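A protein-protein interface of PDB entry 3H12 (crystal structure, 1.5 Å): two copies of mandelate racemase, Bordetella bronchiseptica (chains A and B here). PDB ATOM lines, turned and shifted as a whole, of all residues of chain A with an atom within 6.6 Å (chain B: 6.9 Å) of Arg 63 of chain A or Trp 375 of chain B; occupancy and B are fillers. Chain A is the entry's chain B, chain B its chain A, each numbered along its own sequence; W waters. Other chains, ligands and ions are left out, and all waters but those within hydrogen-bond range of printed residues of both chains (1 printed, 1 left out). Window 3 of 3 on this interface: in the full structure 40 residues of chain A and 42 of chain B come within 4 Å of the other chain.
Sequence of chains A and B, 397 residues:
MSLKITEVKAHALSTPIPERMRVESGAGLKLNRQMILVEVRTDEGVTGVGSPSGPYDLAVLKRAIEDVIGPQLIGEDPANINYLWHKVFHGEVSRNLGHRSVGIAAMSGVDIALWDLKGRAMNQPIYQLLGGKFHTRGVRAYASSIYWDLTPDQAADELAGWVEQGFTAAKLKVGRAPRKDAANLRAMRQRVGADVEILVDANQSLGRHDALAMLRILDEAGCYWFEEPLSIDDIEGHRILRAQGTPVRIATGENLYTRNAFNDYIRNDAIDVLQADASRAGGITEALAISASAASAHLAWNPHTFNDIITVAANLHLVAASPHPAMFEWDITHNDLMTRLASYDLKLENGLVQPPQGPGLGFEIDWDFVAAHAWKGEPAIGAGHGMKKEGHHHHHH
The side-chain carboxylate (OD1) of Asp 57 of chain B is in salt-bridge range of the guanidinium group (NH2) of Arg 63 of chain A (2.8 Å).
The backbone carbonyl oxygen (O) of Ala 12 of chain B lies within hydrogen-bond range of the backbone NH (N) of Trp 375 of chain B (2.9 Å).
NH1 of Arg 63 of chain A is in salt-bridge range of OD2 of Asp 67 of chain A (3.4 Å).
The backbone carbonyl oxygen of Arg 63 of chain A lies within hydrogen-bond range of the backbone NH of Val 68 of chain A (3.5 Å).
The side-chain carboxylate of Asp 57 of chain B sits at hydrogen-bond distance from the backbone NH of Val 60 of chain B (3.0 Å).
OD2 of Asp 57 of chain B lies within hydrogen-bond range of N of Ala 59 of chain B (3.0 Å).
The indole nitrogen (NE1) of Trp 375 of chain B is in hydrogen-bond range of the backbone carbonyl oxygen (O) of Glu 378 of chain B (2.9 Å).
Among the printed residues, pairs that only touch across the chains: Ala 59 of chain A with Arg 63 of chain B (3.5 Å), Val 60 of chain A with Arg 63 of chain B (3.7 Å), Arg 63 of chain A with Ala 59 of chain B (3.4 Å), Arg 63 of chain A with Val 60 of chain B (3.7 Å), Arg 63 of chain A with Trp 375 of chain B (3.5 Å) and Val 68 of chain A with Asp 57 of chain B (3.7 Å).
Of the printed residues of chain B, Ala 59 of chain A touches Arg 63.
Of the printed residues of chain B, Val 60 of chain A touches Arg 63 (3.7 Å).
Printed residues of chain A within 4 Å of Ala 59 of chain B: Arg 63 (3.4 Å).
Printed residues of chain A within 4 Å of Arg 63 of chain B: Ala 59 and Val 60.
The nearest printed residue of chain B that does not touch Val 68 of chain A is Val 60 of chain B (5.1 Å).
Of the 23 printed residues of chain B, 5 touch a printed residue of chain A.
Among the printed residues, 7 pairs touch across the chains.
Among the printed residues, Asp or Glu carboxylates within 4 Å of a Lys or Arg side-chain nitrogen of the other chain: Arg 63 of chain A with Asp 57 of chain B (2.8 Å).
Ala 59 of chain A touches Arg 63 of chain B, and with the chains exchanged Arg 63 of chain A touches Ala 59 of chain B.
Val 60 of chain A touches Arg 63 of chain B, and with the chains exchanged Arg 63 of chain A touches Val 60 of chain B.
Water W1 lies within hydrogen-bond range of O of Ala 59 of chain B (3.2 Å) and O of Ala 59 of chain A (3.2 Å).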
ATOM      1  N   ALA A  10      34.043 -22.238 -38.090  1.00  0.00           N
ATOM      2  CA  ALA A  10      33.469 -20.872 -38.223  1.00  0.00           C
ATOM      3  C   ALA A  10      34.308 -19.965 -37.294  1.00  0.00           C
ATOM      4  O   ALA A  10      34.263 -20.100 -36.097  1.00  0.00           O
ATOM      5  CB  ALA A  10      31.996 -20.869 -37.796  1.00  0.00           C
ATOM      6  N   LEU A  58      27.336 -13.598 -33.462  1.00  0.00           N
ATOM      7  CA  LEU A  58      28.410 -14.455 -33.951  1.00  0.00           C
ATOM      8  C   LEU A  58      28.368 -15.837 -33.286  1.00  0.00           C
ATOM      9  O   LEU A  58      28.775 -16.831 -33.933  1.00  0.00           O
ATOM     10  CB  LEU A  58      29.799 -13.882 -33.712  1.00  0.00           C
ATOM     11  CG  LEU A  58      30.058 -12.558 -34.476  1.00  0.00           C
ATOM     12  CD1 LEU A  58      31.457 -12.101 -34.096  1.00  0.00           C
ATOM     13  CD2 LEU A  58      30.042 -12.779 -35.997  1.00  0.00           C
ATOM     14  N   ALA A  59      27.973 -15.913 -31.998  1.00  0.00           N
ATOM     15  CA  ALA A  59      27.879 -17.214 -31.321  1.00  0.00           C
ATOM     16  C   ALA A  59      26.781 -18.098 -31.944  1.00  0.00           C
ATOM     17  O   ALA A  59      26.918 -19.327 -32.084  1.00  0.00           O
ATOM     18  CB  ALA A  59      27.711 -17.079 -29.824  1.00  0.00           C
ATOM     19  N   VAL A  60      25.676 -17.455 -32.254  1.00  0.00           N
ATOM     20  CA  VAL A  60      24.578 -18.209 -32.962  1.00  0.00           C
ATOM     21  C   VAL A  60      25.046 -18.704 -34.300  1.00  0.00           C
ATOM     22  O   VAL A  60      24.885 -19.915 -34.594  1.00  0.00           O
ATOM     23  CB  VAL A  60      23.322 -17.294 -33.101  1.00  0.00           C
ATOM     24  CG1 VAL A  60      22.381 -17.996 -34.098  1.00  0.00           C
ATOM     25  CG2 VAL A  60      22.680 -17.057 -31.717  1.00  0.00           C
ATOM     26  N   LEU A  61      25.736 -17.871 -35.075  1.00  0.00           N
ATOM     27  CA  LEU A  61      26.213 -18.315 -36.410  1.00  0.00           C
ATOM     28  C   LEU A  61      27.272 -19.429 -36.234  1.00  0.00           C
ATOM     29  O   LEU A  61      27.221 -20.432 -36.980  1.00  0.00           O
ATOM     30  CB  LEU A  61      26.869 -17.182 -37.193  1.00  0.00           C
ATOM     31  CG  LEU A  61      25.884 -16.147 -37.760  1.00  0.00           C
ATOM     32  CD1 LEU A  61      26.729 -14.990 -38.176  1.00  0.00           C
ATOM     33  CD2 LEU A  61      25.159 -16.779 -38.965  1.00  0.00           C
ATOM     34  N   LYS A  62      28.199 -19.311 -35.238  1.00  0.00           N
ATOM     35  CA  LYS A  62      29.221 -20.334 -35.149  1.00  0.00           C
ATOM     36  C   LYS A  62      28.581 -21.695 -34.779  1.00  0.00           C
ATOM     37  O   LYS A  62      28.961 -22.755 -35.307  1.00  0.00           O
ATOM     38  CB  LYS A  62      30.244 -19.901 -34.069  1.00  0.00           C
ATOM     39  CG  LYS A  62      31.332 -20.923 -33.809  1.00  0.00           C
ATOM     40  CD  LYS A  62      32.312 -20.366 -32.741  1.00  0.00           C
ATOM     41  CE  LYS A  62      33.478 -21.340 -32.428  1.00  0.00           C
ATOM     42  NZ  LYS A  62      34.499 -21.307 -33.521  1.00  0.00           N
ATOM     43  N   ARG A  63      27.617 -21.667 -33.889  1.00  0.00           N
ATOM     44  CA  ARG A  63      27.023 -22.896 -33.364  1.00  0.00           C
ATOM     45  C   ARG A  63      26.290 -23.471 -34.569  1.00  0.00           C
ATOM     46  O   ARG A  63      26.327 -24.693 -34.816  1.00  0.00           O
ATOM     47  CB  ARG A  63      26.035 -22.521 -32.242  1.00  0.00           C
ATOM     48  CG  ARG A  63      25.181 -23.713 -31.721  1.00  0.00           C
ATOM     49  CD  ARG A  63      26.042 -24.900 -31.113  1.00  0.00           C
ATOM     50  NE  ARG A  63      25.093 -26.013 -30.945  1.00  0.00           N
ATOM     51  CZ  ARG A  63      25.458 -27.186 -30.395  1.00  0.00           C
ATOM     52  NH1 ARG A  63      26.729 -27.395 -29.968  1.00  0.00           N
ATOM     53  NH2 ARG A  63      24.499 -28.134 -30.320  1.00  0.00           N
ATOM     54  N   ALA A  64      25.507 -22.637 -35.301  1.00  0.00           N
ATOM     55  CA  ALA A  64      24.740 -23.192 -36.494  1.00  0.00           C
ATOM     56  C   ALA A  64      25.632 -23.837 -37.520  1.00  0.00           C
ATOM     57  O   ALA A  64      25.346 -24.897 -38.049  1.00  0.00           O
ATOM     58  CB  ALA A  64      23.863 -22.059 -37.193  1.00  0.00           C
ATOM     59  N   ILE A  65      26.776 -23.184 -37.799  1.00  0.00           N
ATOM     60  CA  ILE A  65      27.631 -23.670 -38.869  1.00  0.00           C
ATOM     61  C   ILE A  65      28.361 -24.895 -38.430  1.00  0.00           C
ATOM     62  O   ILE A  65      28.394 -25.867 -39.155  1.00  0.00           O
ATOM     63  CB  ILE A  65      28.646 -22.526 -39.236  1.00  0.00           C
ATOM     64  CG1 ILE A  65      27.823 -21.445 -39.994  1.00  0.00           C
ATOM     65  CG2 ILE A  65      29.875 -23.110 -40.074  1.00  0.00           C
ATOM     66  CD1 ILE A  65      28.543 -20.010 -40.137  1.00  0.00           C
ATOM     67  N   GLU A  66      28.946 -24.856 -37.219  1.00  0.00           N
ATOM     68  CA  GLU A  66      29.845 -25.959 -36.834  1.00  0.00           C
ATOM     69  C   GLU A  66      29.031 -27.161 -36.319  1.00  0.00           C
ATOM     70  O   GLU A  66      29.470 -28.333 -36.482  1.00  0.00           O
ATOM     71  CB  GLU A  66      30.827 -25.560 -35.744  1.00  0.00           C
ATOM     72  CG  GLU A  66      31.728 -24.455 -36.198  1.00  0.00           C
ATOM     73  CD  GLU A  66      32.833 -24.098 -35.179  1.00  0.00           C
ATOM     74  OE1 GLU A  66      32.779 -24.509 -33.991  1.00  0.00           O
ATOM     75  OE2 GLU A  66      33.799 -23.424 -35.598  1.00  0.00           O
ATOM     76  N   ASP A  67      27.867 -26.928 -35.713  1.00  0.00           N
ATOM     77  CA  ASP A  67      27.235 -27.992 -34.935  1.00  0.00           C
ATOM     78  C   ASP A  67      25.845 -28.381 -35.450  1.00  0.00           C
ATOM     79  O   ASP A  67      25.319 -29.453 -35.025  1.00  0.00           O
ATOM     80  CB  ASP A  67      27.122 -27.568 -33.443  1.00  0.00           C
ATOM     81  CG  ASP A  67      28.526 -27.344 -32.812  1.00  0.00           C
ATOM     82  OD1 ASP A  67      29.365 -28.295 -32.861  1.00  0.00           O
ATOM     83  OD2 ASP A  67      28.795 -26.202 -32.441  1.00  0.00           O
ATOM     84  N   VAL A  68      25.254 -27.603 -36.337  1.00  0.00           N
ATOM     85  CA  VAL A  68      23.927 -27.929 -36.896  1.00  0.00           C
ATOM     86  C   VAL A  68      24.207 -28.327 -38.376  1.00  0.00           C
ATOM     87  O   VAL A  68      23.907 -29.440 -38.802  1.00  0.00           O
ATOM     88  CB  VAL A  68      22.936 -26.789 -36.794  1.00  0.00           C
ATOM     89  CG1 VAL A  68      21.545 -27.233 -37.471  1.00  0.00           C
ATOM     90  CG2 VAL A  68      22.641 -26.489 -35.339  1.00  0.00           C
ATOM     91  N   ILE A  69      24.822 -27.446 -39.158  1.00  0.00           N
ATOM     92  CA  ILE A  69      25.018 -27.691 -40.581  1.00  0.00           C
ATOM     93  C   ILE A  69      26.258 -28.631 -40.749  1.00  0.00           C
ATOM     94  O   ILE A  69      26.220 -29.646 -41.490  1.00  0.00           O
ATOM     95  CB  ILE A  69      25.288 -26.359 -41.266  1.00  0.00           C
ATOM     96  CG1 ILE A  69      23.992 -25.567 -41.235  1.00  0.00           C
ATOM     97  CG2 ILE A  69      25.791 -26.647 -42.667  1.00  0.00           C
ATOM     98  CD1 ILE A  69      24.229 -24.108 -41.653  1.00  0.00           C
ATOM     99  N   GLY A  70      27.359 -28.286 -40.065  1.00  0.00           N
ATOM    100  CA  GLY A  70      28.626 -29.067 -40.237  1.00  0.00           C
ATOM    101  C   GLY A  70      28.478 -30.587 -40.191  1.00  0.00           C
ATOM    102  O   GLY A  70      29.049 -31.278 -41.080  1.00  0.00           O
ATOM    103  N   HIS B  11      17.773 -22.433 -19.217  1.00  0.00           N
ATOM    104  CA  HIS B  11      18.272 -23.772 -18.761  1.00  0.00           C
ATOM    105  C   HIS B  11      18.021 -24.767 -19.888  1.00  0.00           C
ATOM    106  O   HIS B  11      16.848 -25.136 -20.137  1.00  0.00           O
ATOM    107  CB  HIS B  11      17.538 -24.221 -17.512  1.00  0.00           C
ATOM    108  CG  HIS B  11      17.670 -23.279 -16.367  1.00  0.00           C
ATOM    109  ND1 HIS B  11      16.737 -22.311 -16.043  1.00  0.00           N
ATOM    110  CD2 HIS B  11      18.560 -23.280 -15.354  1.00  0.00           C
ATOM    111  CE1 HIS B  11      17.115 -21.666 -14.951  1.00  0.00           C
ATOM    112  NE2 HIS B  11      18.198 -22.267 -14.484  1.00  0.00           N
ATOM    113  N   ALA B  12      19.134 -25.274 -20.455  1.00  0.00           N
ATOM    114  CA  ALA B  12      19.039 -26.271 -21.503  1.00  0.00           C
ATOM    115  C   ALA B  12      18.819 -27.645 -20.820  1.00  0.00           C
ATOM    116  O   ALA B  12      19.680 -28.095 -20.006  1.00  0.00           O
ATOM    117  CB  ALA B  12      20.290 -26.251 -22.329  1.00  0.00           C
ATOM    118  N   LEU B  13      17.736 -28.327 -21.162  1.00  0.00           N
ATOM    119  CA  LEU B  13      17.319 -29.624 -20.531  1.00  0.00           C
ATOM    120  C   LEU B  13      17.185 -30.718 -21.569  1.00  0.00           C
ATOM    121  O   LEU B  13      16.712 -30.467 -22.697  1.00  0.00           O
ATOM    122  CB  LEU B  13      16.011 -29.539 -19.660  1.00  0.00           C
ATOM    123  CG  LEU B  13      16.026 -28.384 -18.683  1.00  0.00           C
ATOM    124  CD1 LEU B  13      14.689 -28.547 -18.078  1.00  0.00           C
ATOM    125  CD2 LEU B  13      17.199 -28.622 -17.677  1.00  0.00           C
ATOM    126  N   SER B  14      17.603 -31.937 -21.244  1.00  0.00           N
ATOM    127  CA  SER B  14      17.355 -33.053 -22.162  1.00  0.00           C
ATOM    128  C   SER B  14      16.836 -34.220 -21.345  1.00  0.00           C
ATOM    129  O   SER B  14      17.294 -34.463 -20.201  1.00  0.00           O
ATOM    130  CB  SER B  14      18.602 -33.399 -22.915  1.00  0.00           C
ATOM    131  OG  SER B  14      18.395 -34.401 -23.943  1.00  0.00           O
ATOM    132  N   GLN B  34      13.642 -32.436 -25.453  1.00  0.00           N
ATOM    133  CA  GLN B  34      14.434 -31.346 -24.916  1.00  0.00           C
ATOM    134  C   GLN B  34      13.597 -30.105 -24.772  1.00  0.00           C
ATOM    135  O   GLN B  34      12.545 -29.965 -25.405  1.00  0.00           O
ATOM    136  CB  GLN B  34      15.614 -31.103 -25.848  1.00  0.00           C
ATOM    137  CG  GLN B  34      16.462 -32.388 -26.077  1.00  0.00           C
ATOM    138  CD  GLN B  34      17.717 -32.138 -26.872  1.00  0.00           C
ATOM    139  OE1 GLN B  34      17.832 -31.196 -27.705  1.00  0.00           O
ATOM    140  NE2 GLN B  34      18.735 -32.945 -26.534  1.00  0.00           N
ATOM    141  N   MET B  35      14.150 -29.159 -24.015  1.00  0.00           N
ATOM    142  CA  MET B  35      13.558 -27.833 -23.886  1.00  0.00           C
ATOM    143  C   MET B  35      14.606 -26.882 -23.376  1.00  0.00           C
ATOM    144  O   MET B  35      15.589 -27.288 -22.752  1.00  0.00           O
ATOM    145  CB  MET B  35      12.294 -27.795 -23.008  1.00  0.00           C
ATOM    146  CG  MET B  35      12.566 -28.091 -21.498  1.00  0.00           C
ATOM    147  SD  MET B  35      11.171 -28.102 -20.325  1.00  0.00           S
ATOM    148  CE  MET B  35      10.506 -26.328 -20.527  1.00  0.00           C
ATOM    149  N   ILE B  36      14.298 -25.585 -23.530  1.00  0.00           N
ATOM    150  CA  ILE B  36      14.890 -24.556 -22.722  1.00  0.00           C
ATOM    151  C   ILE B  36      13.820 -24.181 -21.707  1.00  0.00           C
ATOM    152  O   ILE B  36      12.660 -23.886 -22.041  1.00  0.00           O
ATOM    153  CB  ILE B  36      15.231 -23.270 -23.524  1.00  0.00           C
ATOM    154  CG1 ILE B  36      16.369 -23.545 -24.458  1.00  0.00           C
ATOM    155  CG2 ILE B  36      15.502 -22.130 -22.589  1.00  0.00           C
ATOM    156  CD1 ILE B  36      17.740 -23.720 -23.793  1.00  0.00           C
ATOM    157  N   ASP B  57      18.007 -25.976 -31.844  1.00  0.00           N
ATOM    158  CA  ASP B  57      19.260 -26.338 -31.238  1.00  0.00           C
ATOM    159  C   ASP B  57      19.294 -25.596 -29.876  1.00  0.00           C
ATOM    160  O   ASP B  57      18.960 -24.375 -29.795  1.00  0.00           O
ATOM    161  CB  ASP B  57      20.389 -25.824 -32.124  1.00  0.00           C
ATOM    162  CG  ASP B  57      21.718 -26.166 -31.553  1.00  0.00           C
ATOM    163  OD1 ASP B  57      22.178 -27.313 -31.717  1.00  0.00           O
ATOM    164  OD2 ASP B  57      22.247 -25.371 -30.745  1.00  0.00           O
ATOM    165  N   LEU B  58      19.629 -26.304 -28.799  1.00  0.00           N
ATOM    166  CA  LEU B  58      19.535 -25.672 -27.479  1.00  0.00           C
ATOM    167  C   LEU B  58      20.587 -24.608 -27.262  1.00  0.00           C
ATOM    168  O   LEU B  58      20.253 -23.673 -26.508  1.00  0.00           O
ATOM    169  CB  LEU B  58      19.667 -26.717 -26.342  1.00  0.00           C
ATOM    170  CG  LEU B  58      18.560 -27.779 -26.264  1.00  0.00           C
ATOM    171  CD1 LEU B  58      18.757 -28.725 -25.056  1.00  0.00           C
ATOM    172  CD2 LEU B  58      17.240 -27.017 -25.994  1.00  0.00           C
ATOM    173  N   ALA B  59      21.812 -24.757 -27.845  1.00  0.00           N
ATOM    174  CA  ALA B  59      22.805 -23.711 -27.687  1.00  0.00           C
ATOM    175  C   ALA B  59      22.365 -22.489 -28.426  1.00  0.00           C
ATOM    176  O   ALA B  59      22.596 -21.349 -27.895  1.00  0.00           O
ATOM    177  CB  ALA B  59      24.170 -24.194 -28.165  1.00  0.00           C
ATOM    178  N   VAL B  60      21.794 -22.619 -29.620  1.00  0.00           N
ATOM    179  CA  VAL B  60      21.305 -21.406 -30.321  1.00  0.00           C
ATOM    180  C   VAL B  60      20.199 -20.718 -29.518  1.00  0.00           C
ATOM    181  O   VAL B  60      20.252 -19.478 -29.322  1.00  0.00           O
ATOM    182  CB  VAL B  60      20.718 -21.820 -31.678  1.00  0.00           C
ATOM    183  CG1 VAL B  60      19.925 -20.638 -32.293  1.00  0.00           C
ATOM    184  CG2 VAL B  60      21.934 -22.240 -32.585  1.00  0.00           C
ATOM    185  N   LEU B  61      19.286 -21.487 -28.961  1.00  0.00           N
ATOM    186  CA  LEU B  61      18.179 -20.876 -28.166  1.00  0.00           C
ATOM    187  C   LEU B  61      18.760 -20.204 -26.893  1.00  0.00           C
ATOM    188  O   LEU B  61      18.306 -19.111 -26.516  1.00  0.00           O
ATOM    189  CB  LEU B  61      17.158 -21.909 -27.657  1.00  0.00           C
ATOM    190  CG  LEU B  61      16.154 -22.407 -28.696  1.00  0.00           C
ATOM    191  CD1 LEU B  61      15.458 -23.644 -28.265  1.00  0.00           C
ATOM    192  CD2 LEU B  61      15.137 -21.260 -29.074  1.00  0.00           C
ATOM    193  N   LYS B  62      19.730 -20.883 -26.216  1.00  0.00           N
ATOM    194  CA  LYS B  62      20.247 -20.296 -24.951  1.00  0.00           C
ATOM    195  C   LYS B  62      20.933 -18.970 -25.241  1.00  0.00           C
ATOM    196  O   LYS B  62      20.795 -17.994 -24.513  1.00  0.00           O
ATOM    197  CB  LYS B  62      21.205 -21.288 -24.278  1.00  0.00           C
ATOM    198  CG  LYS B  62      21.768 -20.788 -22.945  1.00  0.00           C
ATOM    199  CD  LYS B  62      22.737 -21.841 -22.392  1.00  0.00           C
ATOM    200  CE  LYS B  62      23.464 -21.420 -21.088  1.00  0.00           C
ATOM    201  NZ  LYS B  62      22.492 -21.332 -19.981  1.00  0.00           N
ATOM    202  N   ARG B  63      21.696 -18.947 -26.317  1.00  0.00           N
ATOM    203  CA  ARG B  63      22.481 -17.719 -26.626  1.00  0.00           C
ATOM    204  C   ARG B  63      21.435 -16.650 -27.020  1.00  0.00           C
ATOM    205  O   ARG B  63      21.584 -15.449 -26.679  1.00  0.00           O
ATOM    206  CB  ARG B  63      23.380 -17.986 -27.810  1.00  0.00           C
ATOM    207  CG  ARG B  63      24.096 -16.781 -28.358  1.00  0.00           C
ATOM    208  CD  ARG B  63      25.172 -16.254 -27.430  1.00  0.00           C
ATOM    209  NE  ARG B  63      25.631 -14.958 -27.980  1.00  0.00           N
ATOM    210  CZ  ARG B  63      26.510 -14.145 -27.402  1.00  0.00           C
ATOM    211  NH1 ARG B  63      26.979 -14.440 -26.208  1.00  0.00           N
ATOM    212  NH2 ARG B  63      26.857 -12.968 -27.970  1.00  0.00           N
ATOM    213  N   VAL B 370      14.879 -30.178 -12.828  1.00  0.00           N
ATOM    214  CA  VAL B 370      15.637 -29.328 -13.754  1.00  0.00           C
ATOM    215  C   VAL B 370      17.125 -29.513 -13.531  1.00  0.00           C
ATOM    216  O   VAL B 370      17.906 -29.753 -14.486  1.00  0.00           O
ATOM    217  CB  VAL B 370      15.270 -27.866 -13.450  1.00  0.00           C
ATOM    218  CG1 VAL B 370      16.165 -26.879 -14.173  1.00  0.00           C
ATOM    219  CG2 VAL B 370      13.738 -27.597 -13.738  1.00  0.00           C
ATOM    220  N   HIS B 373      18.695 -32.749 -15.180  1.00  0.00           N
ATOM    221  CA  HIS B 373      18.604 -33.048 -16.614  1.00  0.00           C
ATOM    222  C   HIS B 373      19.245 -31.997 -17.449  1.00  0.00           C
ATOM    223  O   HIS B 373      18.752 -31.684 -18.536  1.00  0.00           O
ATOM    224  CB  HIS B 373      17.107 -33.215 -17.024  1.00  0.00           C
ATOM    225  CG  HIS B 373      16.474 -34.357 -16.283  1.00  0.00           C
ATOM    226  ND1 HIS B 373      16.434 -35.678 -16.753  1.00  0.00           N
ATOM    227  CD2 HIS B 373      16.165 -34.415 -14.965  1.00  0.00           C
ATOM    228  CE1 HIS B 373      16.025 -36.470 -15.755  1.00  0.00           C
ATOM    229  NE2 HIS B 373      15.801 -35.723 -14.694  1.00  0.00           N
ATOM    230  N   ALA B 374      20.396 -31.485 -17.021  1.00  0.00           N
ATOM    231  CA  ALA B 374      21.119 -30.539 -17.929  1.00  0.00           C
ATOM    232  C   ALA B 374      21.475 -31.208 -19.187  1.00  0.00           C
ATOM    233  O   ALA B 374      21.853 -32.385 -19.188  1.00  0.00           O
ATOM    234  CB  ALA B 374      22.396 -29.982 -17.257  1.00  0.00           C
ATOM    235  N   TRP B 375      21.187 -30.536 -20.313  1.00  0.00           N
ATOM    236  CA  TRP B 375      21.696 -30.976 -21.589  1.00  0.00           C
ATOM    237  C   TRP B 375      23.185 -31.180 -21.672  1.00  0.00           C
ATOM    238  O   TRP B 375      23.957 -30.326 -21.159  1.00  0.00           O
ATOM    239  CB  TRP B 375      21.311 -29.910 -22.631  1.00  0.00           C
ATOM    240  CG  TRP B 375      21.733 -30.179 -24.039  1.00  0.00           C
ATOM    241  CD1 TRP B 375      21.378 -31.211 -24.844  1.00  0.00           C
ATOM    242  CD2 TRP B 375      22.407 -29.238 -24.860  1.00  0.00           C
ATOM    243  NE1 TRP B 375      21.856 -31.008 -26.130  1.00  0.00           N
ATOM    244  CE2 TRP B 375      22.464 -29.777 -26.156  1.00  0.00           C
ATOM    245  CE3 TRP B 375      22.974 -27.981 -24.626  1.00  0.00           C
ATOM    246  CZ2 TRP B 375      23.095 -29.112 -27.203  1.00  0.00           C
ATOM    247  CZ3 TRP B 375      23.567 -27.277 -25.692  1.00  0.00           C
ATOM    248  CH2 TRP B 375      23.615 -27.843 -26.968  1.00  0.00           C
ATOM    249  N   LYS B 376      23.594 -32.280 -22.274  1.00  0.00           N
ATOM    250  CA  LYS B 376      25.029 -32.555 -22.496  1.00  0.00           C
ATOM    251  C   LYS B 376      25.454 -32.679 -23.982  1.00  0.00           C
ATOM    252  O   LYS B 376      26.493 -33.290 -24.310  1.00  0.00           O
ATOM    253  CB  LYS B 376      25.445 -33.773 -21.635  1.00  0.00           C
ATOM    254  CG  LYS B 376      25.676 -33.222 -20.269  1.00  0.00           C
ATOM    255  CD  LYS B 376      24.927 -33.986 -19.305  1.00  0.00           C
ATOM    256  CE  LYS B 376      25.705 -34.155 -17.992  1.00  0.00           C
ATOM    257  NZ  LYS B 376      25.313 -35.545 -17.382  1.00  0.00           N
ATOM    258  N   GLY B 377      24.673 -32.091 -24.913  1.00  0.00           N
ATOM    259  CA  GLY B 377      25.015 -32.053 -26.307  1.00  0.00           C
ATOM    260  C   GLY B 377      24.226 -33.109 -27.111  1.00  0.00           C
ATOM    261  O   GLY B 377      24.471 -33.222 -28.286  1.00  0.00           O
ATOM    262  N   GLU B 378      23.339 -33.887 -26.471  1.00  0.00           N
ATOM    263  CA  GLU B 378      22.499 -34.900 -27.149  1.00  0.00           C
ATOM    264  C   GLU B 378      21.681 -34.214 -28.240  1.00  0.00           C
ATOM    265  O   GLU B 378      21.253 -33.019 -28.091  1.00  0.00           O
ATOM    266  CB  GLU B 378      21.474 -35.501 -26.180  1.00  0.00           C
ATOM    267  CG  GLU B 378      22.012 -36.261 -24.970  1.00  0.00           C
ATOM    268  CD  GLU B 378      22.185 -35.398 -23.702  1.00  0.00           C
ATOM    269  OE1 GLU B 378      22.301 -34.176 -23.766  1.00  0.00           O
ATOM    270  OE2 GLU B 378      22.275 -36.002 -22.621  1.00  0.00           O
ATOM    271  N   PRO B 379      21.411 -34.960 -29.339  1.00  0.00           N
ATOM    272  CA  PRO B 379      20.541 -34.433 -30.410  1.00  0.00           C
ATOM    273  C   PRO B 379      19.050 -34.628 -30.015  1.00  0.00           C
ATOM    274  O   PRO B 379      18.737 -35.581 -29.312  1.00  0.00           O
ATOM    275  CB  PRO B 379      20.928 -35.357 -31.604  1.00  0.00           C
ATOM    276  CG  PRO B 379      21.227 -36.762 -30.925  1.00  0.00           C
ATOM    277  CD  PRO B 379      21.914 -36.339 -29.591  1.00  0.00           C
ATOM    278  N   ALA B 380      18.125 -33.755 -30.404  1.00  0.00           N
ATOM    279  CA  ALA B 380      16.687 -33.950 -30.067  1.00  0.00           C
ATOM    280  C   ALA B 380      16.042 -34.942 -31.106  1.00  0.00           C
ATOM    281  O   ALA B 380      15.165 -35.705 -30.776  1.00  0.00           O
ATOM    282  CB  ALA B 380      15.959 -32.600 -30.105  1.00  0.00           C
HETATM  283  O   HOH W   1      24.707 -20.337 -30.011  1.00  0.00           O
